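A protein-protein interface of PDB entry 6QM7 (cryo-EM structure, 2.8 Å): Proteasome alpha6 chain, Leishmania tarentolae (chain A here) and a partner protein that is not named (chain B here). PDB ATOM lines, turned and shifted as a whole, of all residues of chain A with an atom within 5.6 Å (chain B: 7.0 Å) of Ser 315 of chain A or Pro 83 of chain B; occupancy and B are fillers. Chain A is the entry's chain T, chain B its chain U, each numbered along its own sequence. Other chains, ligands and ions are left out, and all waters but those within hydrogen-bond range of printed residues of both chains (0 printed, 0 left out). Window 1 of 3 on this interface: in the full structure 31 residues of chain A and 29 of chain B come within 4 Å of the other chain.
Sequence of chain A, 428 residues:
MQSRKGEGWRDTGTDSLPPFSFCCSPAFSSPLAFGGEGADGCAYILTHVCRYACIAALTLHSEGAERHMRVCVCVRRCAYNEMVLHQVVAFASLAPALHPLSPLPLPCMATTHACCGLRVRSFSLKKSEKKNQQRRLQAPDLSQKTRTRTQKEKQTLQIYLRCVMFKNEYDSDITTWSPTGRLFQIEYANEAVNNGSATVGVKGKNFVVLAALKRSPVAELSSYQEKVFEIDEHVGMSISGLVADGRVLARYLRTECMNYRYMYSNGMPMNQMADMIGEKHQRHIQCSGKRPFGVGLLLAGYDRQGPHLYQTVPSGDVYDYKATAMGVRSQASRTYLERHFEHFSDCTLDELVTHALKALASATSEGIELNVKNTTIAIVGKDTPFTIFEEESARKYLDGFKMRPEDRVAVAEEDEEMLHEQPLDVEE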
ATOM      1  N   ILE A 186     -16.888  20.961  18.248  1.00  0.00           N
ATOM      2  CA  ILE A 186     -17.966  21.646  17.475  1.00  0.00           C
ATOM      3  C   ILE A 186     -17.343  22.391  16.297  1.00  0.00           C
ATOM      4  O   ILE A 186     -17.934  22.320  15.219  1.00  0.00           O
ATOM      5  CB  ILE A 186     -18.818  22.555  18.378  1.00  0.00           C
ATOM      6  CG1 ILE A 186     -19.530  21.738  19.454  1.00  0.00           C
ATOM      7  CG2 ILE A 186     -19.807  23.375  17.567  1.00  0.00           C
ATOM      8  CD1 ILE A 186     -20.327  22.576  20.428  1.00  0.00           C
ATOM      9  N   ASN A 190     -18.011  21.453  12.340  1.00  0.00           N
ATOM     10  CA  ASN A 190     -18.309  22.534  11.363  1.00  0.00           C
ATOM     11  C   ASN A 190     -17.452  22.349  10.110  1.00  0.00           C
ATOM     12  O   ASN A 190     -17.951  22.688   9.029  1.00  0.00           O
ATOM     13  CB  ASN A 190     -18.125  23.939  11.944  1.00  0.00           C
ATOM     14  CG  ASN A 190     -19.445  24.600  12.270  1.00  0.00           C
ATOM     15  OD1 ASN A 190     -19.975  24.453  13.377  1.00  0.00           O
ATOM     16  ND2 ASN A 190     -19.991  25.317  11.299  1.00  0.00           N
ATOM     17  N   GLY A 278     -32.396  22.639  16.096  1.00  0.00           N
ATOM     18  CA  GLY A 278     -31.561  23.351  17.079  1.00  0.00           C
ATOM     19  C   GLY A 278     -31.447  22.558  18.365  1.00  0.00           C
ATOM     20  O   GLY A 278     -30.312  22.230  18.742  1.00  0.00           O
ATOM     21  N   GLU A 279     -32.586  22.235  18.987  1.00  0.00           N
ATOM     22  CA  GLU A 279     -32.660  21.506  20.281  1.00  0.00           C
ATOM     23  C   GLU A 279     -31.957  20.162  20.145  1.00  0.00           C
ATOM     24  O   GLU A 279     -31.213  19.807  21.064  1.00  0.00           O
ATOM     25  CB  GLU A 279     -34.101  21.256  20.731  1.00  0.00           C
ATOM     26  CG  GLU A 279     -34.743  22.458  21.417  1.00  0.00           C
ATOM     27  CD  GLU A 279     -34.699  22.458  22.944  1.00  0.00           C
ATOM     28  OE1 GLU A 279     -33.807  23.141  23.520  1.00  0.00           O
ATOM     29  OE2 GLU A 279     -35.575  21.793  23.561  1.00  0.00           O
ATOM     30  N   HIS A 281     -29.676  19.016  17.892  1.00  0.00           N
ATOM     31  CA  HIS A 281     -28.219  19.275  17.785  1.00  0.00           C
ATOM     32  C   HIS A 281     -27.619  19.514  19.170  1.00  0.00           C
ATOM     33  O   HIS A 281     -26.553  18.957  19.448  1.00  0.00           O
ATOM     34  CB  HIS A 281     -27.941  20.478  16.897  1.00  0.00           C
ATOM     35  CG  HIS A 281     -27.973  20.169  15.445  1.00  0.00           C
ATOM     36  ND1 HIS A 281     -29.137  19.866  14.783  1.00  0.00           N
ATOM     37  CD2 HIS A 281     -26.983  20.127  14.532  1.00  0.00           C
ATOM     38  CE1 HIS A 281     -28.864  19.638  13.515  1.00  0.00           C
ATOM     39  NE2 HIS A 281     -27.543  19.800  13.329  1.00  0.00           N
ATOM     40  N   GLN A 282     -28.271  20.330  19.988  1.00  0.00           N
ATOM     41  CA  GLN A 282     -27.750  20.748  21.312  1.00  0.00           C
ATOM     42  C   GLN A 282     -27.655  19.533  22.238  1.00  0.00           C
ATOM     43  O   GLN A 282     -26.716  19.512  23.045  1.00  0.00           O
ATOM     44  CB  GLN A 282     -28.611  21.840  21.954  1.00  0.00           C
ATOM     45  CG  GLN A 282     -27.907  22.619  23.063  1.00  0.00           C
ATOM     46  CD  GLN A 282     -27.773  21.913  24.396  1.00  0.00           C
ATOM     47  OE1 GLN A 282     -28.666  21.194  24.839  1.00  0.00           O
ATOM     48  NE2 GLN A 282     -26.641  22.118  25.050  1.00  0.00           N
ATOM     49  N   ILE A 285     -24.171  18.135  21.793  1.00  0.00           N
ATOM     50  CA  ILE A 285     -22.925  18.923  22.045  1.00  0.00           C
ATOM     51  C   ILE A 285     -22.579  19.046  23.540  1.00  0.00           C
ATOM     52  O   ILE A 285     -21.655  19.826  23.840  1.00  0.00           O
ATOM     53  CB  ILE A 285     -22.987  20.314  21.387  1.00  0.00           C
ATOM     54  CG1 ILE A 285     -24.047  21.222  22.010  1.00  0.00           C
ATOM     55  CG2 ILE A 285     -23.171  20.186  19.888  1.00  0.00           C
ATOM     56  CD1 ILE A 285     -23.856  22.687  21.702  1.00  0.00           C
ATOM     57  N   VAL A 313     -26.726  24.051  11.606  1.00  0.00           N
ATOM     58  CA  VAL A 313     -25.245  23.940  11.675  1.00  0.00           C
ATOM     59  C   VAL A 313     -24.920  23.050  12.875  1.00  0.00           C
ATOM     60  O   VAL A 313     -25.734  22.946  13.787  1.00  0.00           O
ATOM     61  CB  VAL A 313     -24.668  25.370  11.732  1.00  0.00           C
ATOM     62  CG1 VAL A 313     -24.127  25.750  13.102  1.00  0.00           C
ATOM     63  CG2 VAL A 313     -23.631  25.616  10.647  1.00  0.00           C
ATOM     64  N   PRO A 314     -23.779  22.331  12.907  1.00  0.00           N
ATOM     65  CA  PRO A 314     -23.486  21.369  13.978  1.00  0.00           C
ATOM     66  C   PRO A 314     -23.509  21.912  15.412  1.00  0.00           C
ATOM     67  O   PRO A 314     -23.874  21.175  16.320  1.00  0.00           O
ATOM     68  CB  PRO A 314     -22.043  20.976  13.672  1.00  0.00           C
ATOM     69  CG  PRO A 314     -21.995  21.068  12.177  1.00  0.00           C
ATOM     70  CD  PRO A 314     -22.706  22.377  11.904  1.00  0.00           C
ATOM     71  N   SER A 315     -23.122  23.179  15.567  1.00  0.00           N
ATOM     72  CA  SER A 315     -23.117  23.925  16.851  1.00  0.00           C
ATOM     73  C   SER A 315     -24.510  23.945  17.494  1.00  0.00           C
ATOM     74  O   SER A 315     -24.557  24.160  18.708  1.00  0.00           O
ATOM     75  CB  SER A 315     -22.557  25.332  16.679  1.00  0.00           C
ATOM     76  OG  SER A 315     -23.563  26.275  16.322  1.00  0.00           O
ATOM     77  N   GLY A 316     -25.581  23.755  16.711  1.00  0.00           N
ATOM     78  CA  GLY A 316     -26.989  23.793  17.154  1.00  0.00           C
ATOM     79  C   GLY A 316     -27.642  25.125  16.832  1.00  0.00           C
ATOM     80  O   GLY A 316     -28.855  25.277  17.086  1.00  0.00           O
ATOM     81  N   ASP A 317     -26.869  26.069  16.294  1.00  0.00           N
ATOM     82  CA  ASP A 317     -27.389  27.366  15.797  1.00  0.00           C
ATOM     83  C   ASP A 317     -28.279  27.098  14.594  1.00  0.00           C
ATOM     84  O   ASP A 317     -28.007  26.143  13.851  1.00  0.00           O
ATOM     85  CB  ASP A 317     -26.271  28.338  15.427  1.00  0.00           C
ATOM     86  CG  ASP A 317     -25.764  29.116  16.626  1.00  0.00           C
ATOM     87  OD1 ASP A 317     -24.594  28.886  17.014  1.00  0.00           O
ATOM     88  OD2 ASP A 317     -26.550  29.946  17.164  1.00  0.00           O
ATOM     89  N   TYR A 319     -30.277  29.474  11.586  1.00  0.00           N
ATOM     90  CA  TYR A 319     -30.239  30.823  10.995  1.00  0.00           C
ATOM     91  C   TYR A 319     -31.432  30.945  10.060  1.00  0.00           C
ATOM     92  O   TYR A 319     -31.473  30.185   9.098  1.00  0.00           O
ATOM     93  CB  TYR A 319     -28.901  31.002  10.279  1.00  0.00           C
ATOM     94  CG  TYR A 319     -27.687  30.922  11.171  1.00  0.00           C
ATOM     95  CD1 TYR A 319     -27.183  32.051  11.791  1.00  0.00           C
ATOM     96  CD2 TYR A 319     -27.028  29.724  11.389  1.00  0.00           C
ATOM     97  CE1 TYR A 319     -26.071  31.993  12.620  1.00  0.00           C
ATOM     98  CE2 TYR A 319     -25.910  29.647  12.205  1.00  0.00           C
ATOM     99  CZ  TYR A 319     -25.431  30.787  12.830  1.00  0.00           C
ATOM    100  OH  TYR A 319     -24.337  30.740  13.643  1.00  0.00           O
ATOM    101  N   ARG B  66     -32.075  35.982  20.659  1.00  0.00           N
ATOM    102  CA  ARG B  66     -31.414  35.612  21.933  1.00  0.00           C
ATOM    103  C   ARG B  66     -32.393  35.758  23.095  1.00  0.00           C
ATOM    104  O   ARG B  66     -32.004  35.375  24.194  1.00  0.00           O
ATOM    105  CB  ARG B  66     -30.182  36.480  22.150  1.00  0.00           C
ATOM    106  CG  ARG B  66     -29.230  36.457  20.967  1.00  0.00           C
ATOM    107  CD  ARG B  66     -27.857  36.975  21.327  1.00  0.00           C
ATOM    108  NE  ARG B  66     -27.136  35.929  22.032  1.00  0.00           N
ATOM    109  CZ  ARG B  66     -26.228  35.123  21.496  1.00  0.00           C
ATOM    110  NH1 ARG B  66     -25.649  34.213  22.252  1.00  0.00           N
ATOM    111  NH2 ARG B  66     -25.868  35.232  20.228  1.00  0.00           N
ATOM    112  N   ILE B  78     -30.426  35.269  26.481  1.00  0.00           N
ATOM    113  CA  ILE B  78     -29.187  34.449  26.537  1.00  0.00           C
ATOM    114  C   ILE B  78     -28.023  35.286  26.038  1.00  0.00           C
ATOM    115  O   ILE B  78     -27.983  35.596  24.829  1.00  0.00           O
ATOM    116  CB  ILE B  78     -29.323  33.197  25.675  1.00  0.00           C
ATOM    117  CG1 ILE B  78     -30.530  32.360  26.087  1.00  0.00           C
ATOM    118  CG2 ILE B  78     -28.033  32.397  25.696  1.00  0.00           C
ATOM    119  CD1 ILE B  78     -31.242  31.789  24.895  1.00  0.00           C
ATOM    120  N   GLY B  80     -24.248  34.437  25.423  1.00  0.00           N
ATOM    121  CA  GLY B  80     -23.300  33.309  25.318  1.00  0.00           C
ATOM    122  C   GLY B  80     -23.542  32.461  24.089  1.00  0.00           C
ATOM    123  O   GLY B  80     -23.948  33.028  23.084  1.00  0.00           O
ATOM    124  N   LEU B  81     -23.252  31.160  24.152  1.00  0.00           N
ATOM    125  CA  LEU B  81     -23.634  30.193  23.089  1.00  0.00           C
ATOM    126  C   LEU B  81     -25.153  30.080  23.061  1.00  0.00           C
ATOM    127  O   LEU B  81     -25.733  29.595  24.041  1.00  0.00           O
ATOM    128  CB  LEU B  81     -23.037  28.807  23.343  1.00  0.00           C
ATOM    129  CG  LEU B  81     -21.524  28.659  23.205  1.00  0.00           C
ATOM    130  CD1 LEU B  81     -21.212  27.242  22.748  1.00  0.00           C
ATOM    131  CD2 LEU B  81     -20.907  29.685  22.248  1.00  0.00           C
ATOM    132  N   LEU B  82     -25.753  30.483  21.951  1.00  0.00           N
ATOM    133  CA  LEU B  82     -27.222  30.543  21.803  1.00  0.00           C
ATOM    134  C   LEU B  82     -27.817  29.142  21.950  1.00  0.00           C
ATOM    135  O   LEU B  82     -28.718  28.961  22.765  1.00  0.00           O
ATOM    136  CB  LEU B  82     -27.538  31.204  20.463  1.00  0.00           C
ATOM    137  CG  LEU B  82     -29.012  31.425  20.149  1.00  0.00           C
ATOM    138  CD1 LEU B  82     -29.796  31.875  21.373  1.00  0.00           C
ATOM    139  CD2 LEU B  82     -29.130  32.446  19.028  1.00  0.00           C
ATOM    140  N   PRO B  83     -27.292  28.097  21.271  1.00  0.00           N
ATOM    141  CA  PRO B  83     -27.844  26.747  21.393  1.00  0.00           C
ATOM    142  C   PRO B  83     -27.923  26.247  22.843  1.00  0.00           C
ATOM    143  O   PRO B  83     -28.986  25.787  23.234  1.00  0.00           O
ATOM    144  CB  PRO B  83     -26.868  25.874  20.594  1.00  0.00           C
ATOM    145  CG  PRO B  83     -26.267  26.839  19.606  1.00  0.00           C
ATOM    146  CD  PRO B  83     -26.119  28.125  20.385  1.00  0.00           C
ATOM    147  N   ASP B  84     -26.819  26.340  23.591  1.00  0.00           N
ATOM    148  CA  ASP B  84     -26.773  26.028  25.047  1.00  0.00           C
ATOM    149  C   ASP B  84     -27.886  26.810  25.754  1.00  0.00           C
ATOM    150  O   ASP B  84     -28.679  26.197  26.490  1.00  0.00           O
ATOM    151  CB  ASP B  84     -25.411  26.377  25.656  1.00  0.00           C
ATOM    152  CG  ASP B  84     -24.366  25.268  25.633  1.00  0.00           C
ATOM    153  OD1 ASP B  84     -24.672  24.152  25.160  1.00  0.00           O
ATOM    154  OD2 ASP B  84     -23.239  25.530  26.093  1.00  0.00           O
ATOM    155  N   GLY B  85     -27.946  28.119  25.510  1.00  0.00           N
ATOM    156  CA  GLY B  85     -28.978  29.028  26.039  1.00  0.00           C
ATOM    157  C   GLY B  85     -30.371  28.487  25.831  1.00  0.00           C
ATOM    158  O   GLY B  85     -31.196  28.599  26.744  1.00  0.00           O
ATOM    159  N   ARG B  86     -30.628  27.927  24.659  1.00  0.00           N
ATOM    160  CA  ARG B  86     -31.973  27.429  24.295  1.00  0.00           C
ATOM    161  C   ARG B  86     -32.304  26.178  25.116  1.00  0.00           C
ATOM    162  O   ARG B  86     -33.498  25.940  25.321  1.00  0.00           O
ATOM    163  CB  ARG B  86     -32.064  27.256  22.779  1.00  0.00           C
ATOM    164  CG  ARG B  86     -31.939  28.588  22.055  1.00  0.00           C
ATOM    165  CD  ARG B  86     -32.782  28.690  20.811  1.00  0.00           C
ATOM    166  NE  ARG B  86     -34.192  28.611  21.152  1.00  0.00           N
ATOM    167  CZ  ARG B  86     -35.178  28.572  20.266  1.00  0.00           C
ATOM    168  NH1 ARG B  86     -36.430  28.483  20.683  1.00  0.00           N
ATOM    169  NH2 ARG B  86     -34.914  28.618  18.971  1.00  0.00           N
ATOM    170  N   ALA B  87     -31.311  25.422  25.578  1.00  0.00           N
ATOM    171  CA  ALA B  87     -31.533  24.252  26.455  1.00  0.00           C
ATOM    172  C   ALA B  87     -32.030  24.736  27.815  1.00  0.00           C
ATOM    173  O   ALA B  87     -32.846  24.014  28.435  1.00  0.00           O
ATOM    174  CB  ALA B  87     -30.279  23.442  26.612  1.00  0.00           C
ATOM    175  N   ILE B  88     -31.521  25.886  28.263  1.00  0.00           N
ATOM    176  CA  ILE B  88     -31.889  26.548  29.546  1.00  0.00           C
ATOM    177  C   ILE B  88     -33.280  27.148  29.402  1.00  0.00           C
ATOM    178  O   ILE B  88     -34.094  27.008  30.333  1.00  0.00           O
ATOM    179  CB  ILE B  88     -30.858  27.619  29.906  1.00  0.00           C
ATOM    180  CG1 ILE B  88     -29.538  26.979  30.311  1.00  0.00           C
ATOM    181  CG2 ILE B  88     -31.364  28.556  30.984  1.00  0.00           C
ATOM    182  CD1 ILE B  88     -28.384  27.895  30.056  1.00  0.00           C
ATOM    183  N   ARG B 130     -20.638  19.041  30.331  1.00  0.00           N
ATOM    184  CA  ARG B 130     -19.846  20.283  30.457  1.00  0.00           C
ATOM    185  C   ARG B 130     -20.745  21.401  30.948  1.00  0.00           C
ATOM    186  O   ARG B 130     -21.961  21.359  30.768  1.00  0.00           O
ATOM    187  CB  ARG B 130     -19.209  20.694  29.135  1.00  0.00           C
ATOM    188  CG  ARG B 130     -20.190  20.861  27.993  1.00  0.00           C
ATOM    189  CD  ARG B 130     -19.508  21.500  26.805  1.00  0.00           C
ATOM    190  NE  ARG B 130     -20.459  21.682  25.722  1.00  0.00           N
ATOM    191  CZ  ARG B 130     -21.390  22.624  25.682  1.00  0.00           C
ATOM    192  NH1 ARG B 130     -22.202  22.683  24.641  1.00  0.00           N
ATOM    193  NH2 ARG B 130     -21.518  23.505  26.664  1.00  0.00           N
ATOM    194  N   PHE B 132     -22.679  24.969  30.855  1.00  0.00           N
ATOM    195  CA  PHE B 132     -23.326  25.783  29.801  1.00  0.00           C
ATOM    196  C   PHE B 132     -22.425  26.959  29.456  1.00  0.00           C
ATOM    197  O   PHE B 132     -21.705  27.455  30.329  1.00  0.00           O
ATOM    198  CB  PHE B 132     -24.709  26.258  30.224  1.00  0.00           C
ATOM    199  CG  PHE B 132     -25.720  25.151  30.211  1.00  0.00           C
ATOM    200  CD1 PHE B 132     -26.013  24.444  31.357  1.00  0.00           C
ATOM    201  CD2 PHE B 132     -26.347  24.791  29.041  1.00  0.00           C
ATOM    202  CE1 PHE B 132     -26.939  23.415  31.342  1.00  0.00           C
ATOM    203  CE2 PHE B 132     -27.287  23.776  29.029  1.00  0.00           C
ATOM    204  CZ  PHE B 132     -27.574  23.078  30.174  1.00  0.00           C
ATOM    205  N   CYS B 134     -23.404  29.903  28.368  1.00  0.00           N
ATOM    206  CA  CYS B 134     -24.257  31.114  28.374  1.00  0.00           C
ATOM    207  C   CYS B 134     -24.610  31.520  29.801  1.00  0.00           C
ATOM    208  O   CYS B 134     -24.761  30.633  30.643  1.00  0.00           O
ATOM    209  CB  CYS B 134     -25.556  30.848  27.640  1.00  0.00           C
ATOM    210  SG  CYS B 134     -26.382  29.374  28.281  1.00  0.00           S
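Printed residues of chain B that touch a printed residue of chain A: Leu 82, Pro 83, Asp 84, Arg 86, Ala 87 and Arg 130.
Of the 13 printed residues of chain A, 6 touch a printed residue of chain B.
Hydrophobic or aromatic side chains of chain A within 4 Å of the printed part of chain B: Ile 285.
Among the printed residues, no Asp or Glu carboxylate lies within 4 Å of a Lys or Arg side-chain nitrogen of the other chain.
Ser 315 of chain A touches one residue of chain B.
Printed residues of chain A within 4 Å of Pro 83 of chain B: Gln 282 (3.4 Å), Ser 315 (3.3 Å), Gly 316 (3.5 Å) and Asp 317 (3.5 Å).
Printed residues of chain A within 4 Å of Arg 86 of chain B: Glu 279.
Printed residues of chain A within 4 Å of Asp 84 of chain B: Gln 282 and Ile 285.
Printed residues of chain B within 4 Å of Glu 279 of chain A: Arg 86 (3.3 Å) and Ala 87 (3.9 Å).
Of the printed residues of chain A, Leu 82 of chain B touches Asp 317 (3.7 Å).
Gly 278 of chain A touches none of the printed residues of chain B.
Leu 81 of chain B touches none of the printed residues of chain A.
The nearest residue of chain B that does not touch Ser 315 of chain A is Asp 84 of chain B (5.8 Å).
The nearest residue of chain A that does not touch Pro 83 of chain B is Ile 285 of chain A (4.5 Å).
The nearest printed residue of chain A that does not touch Leu 82 of chain B is Gly 316 of chain A (6.3 Å).
Among the printed residues, merely in contact across the chains: Glu 279 of chain A with Ala 87 of chain B, Gln 282 of chain A with Pro 83 of chain B, Gln 282 of chain A with Ala 87 of chain B, Ile 285 of chain A with Asp 84 of chain B, Ser 315 of chain A with Pro 83 of chain B, Gly 316 of chain A with Pro 83 of chain B, Asp 317 of chain A with Leu 82 of chain B and Asp 317 of chain A with Pro 83 of chain B.
NH2 of Arg 130 of chain B is in salt-bridge range of OD2 of Asp 84 of chain B, 2.7 Å away.
OD1 of Asp 317 of chain A sits at hydrogen-bond distance from OG of Ser 315 of chain A (2.9 Å).
The side-chain amide nitrogen of Gln 282 of chain A sits at hydrogen-bond distance from the side-chain carboxylate of Asp 84 of chain B.
The side-chain carboxylate of Glu 279 of chain A sits close to the backbone carbonyl oxygen of Arg 86 of chain B (3.3 Å).
The backbone carbonyl oxygen (O) of Ile 285 of chain A is in hydrogen-bond range of the guanidinium group (NE) of Arg 130 of chain B (2.9 Å).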
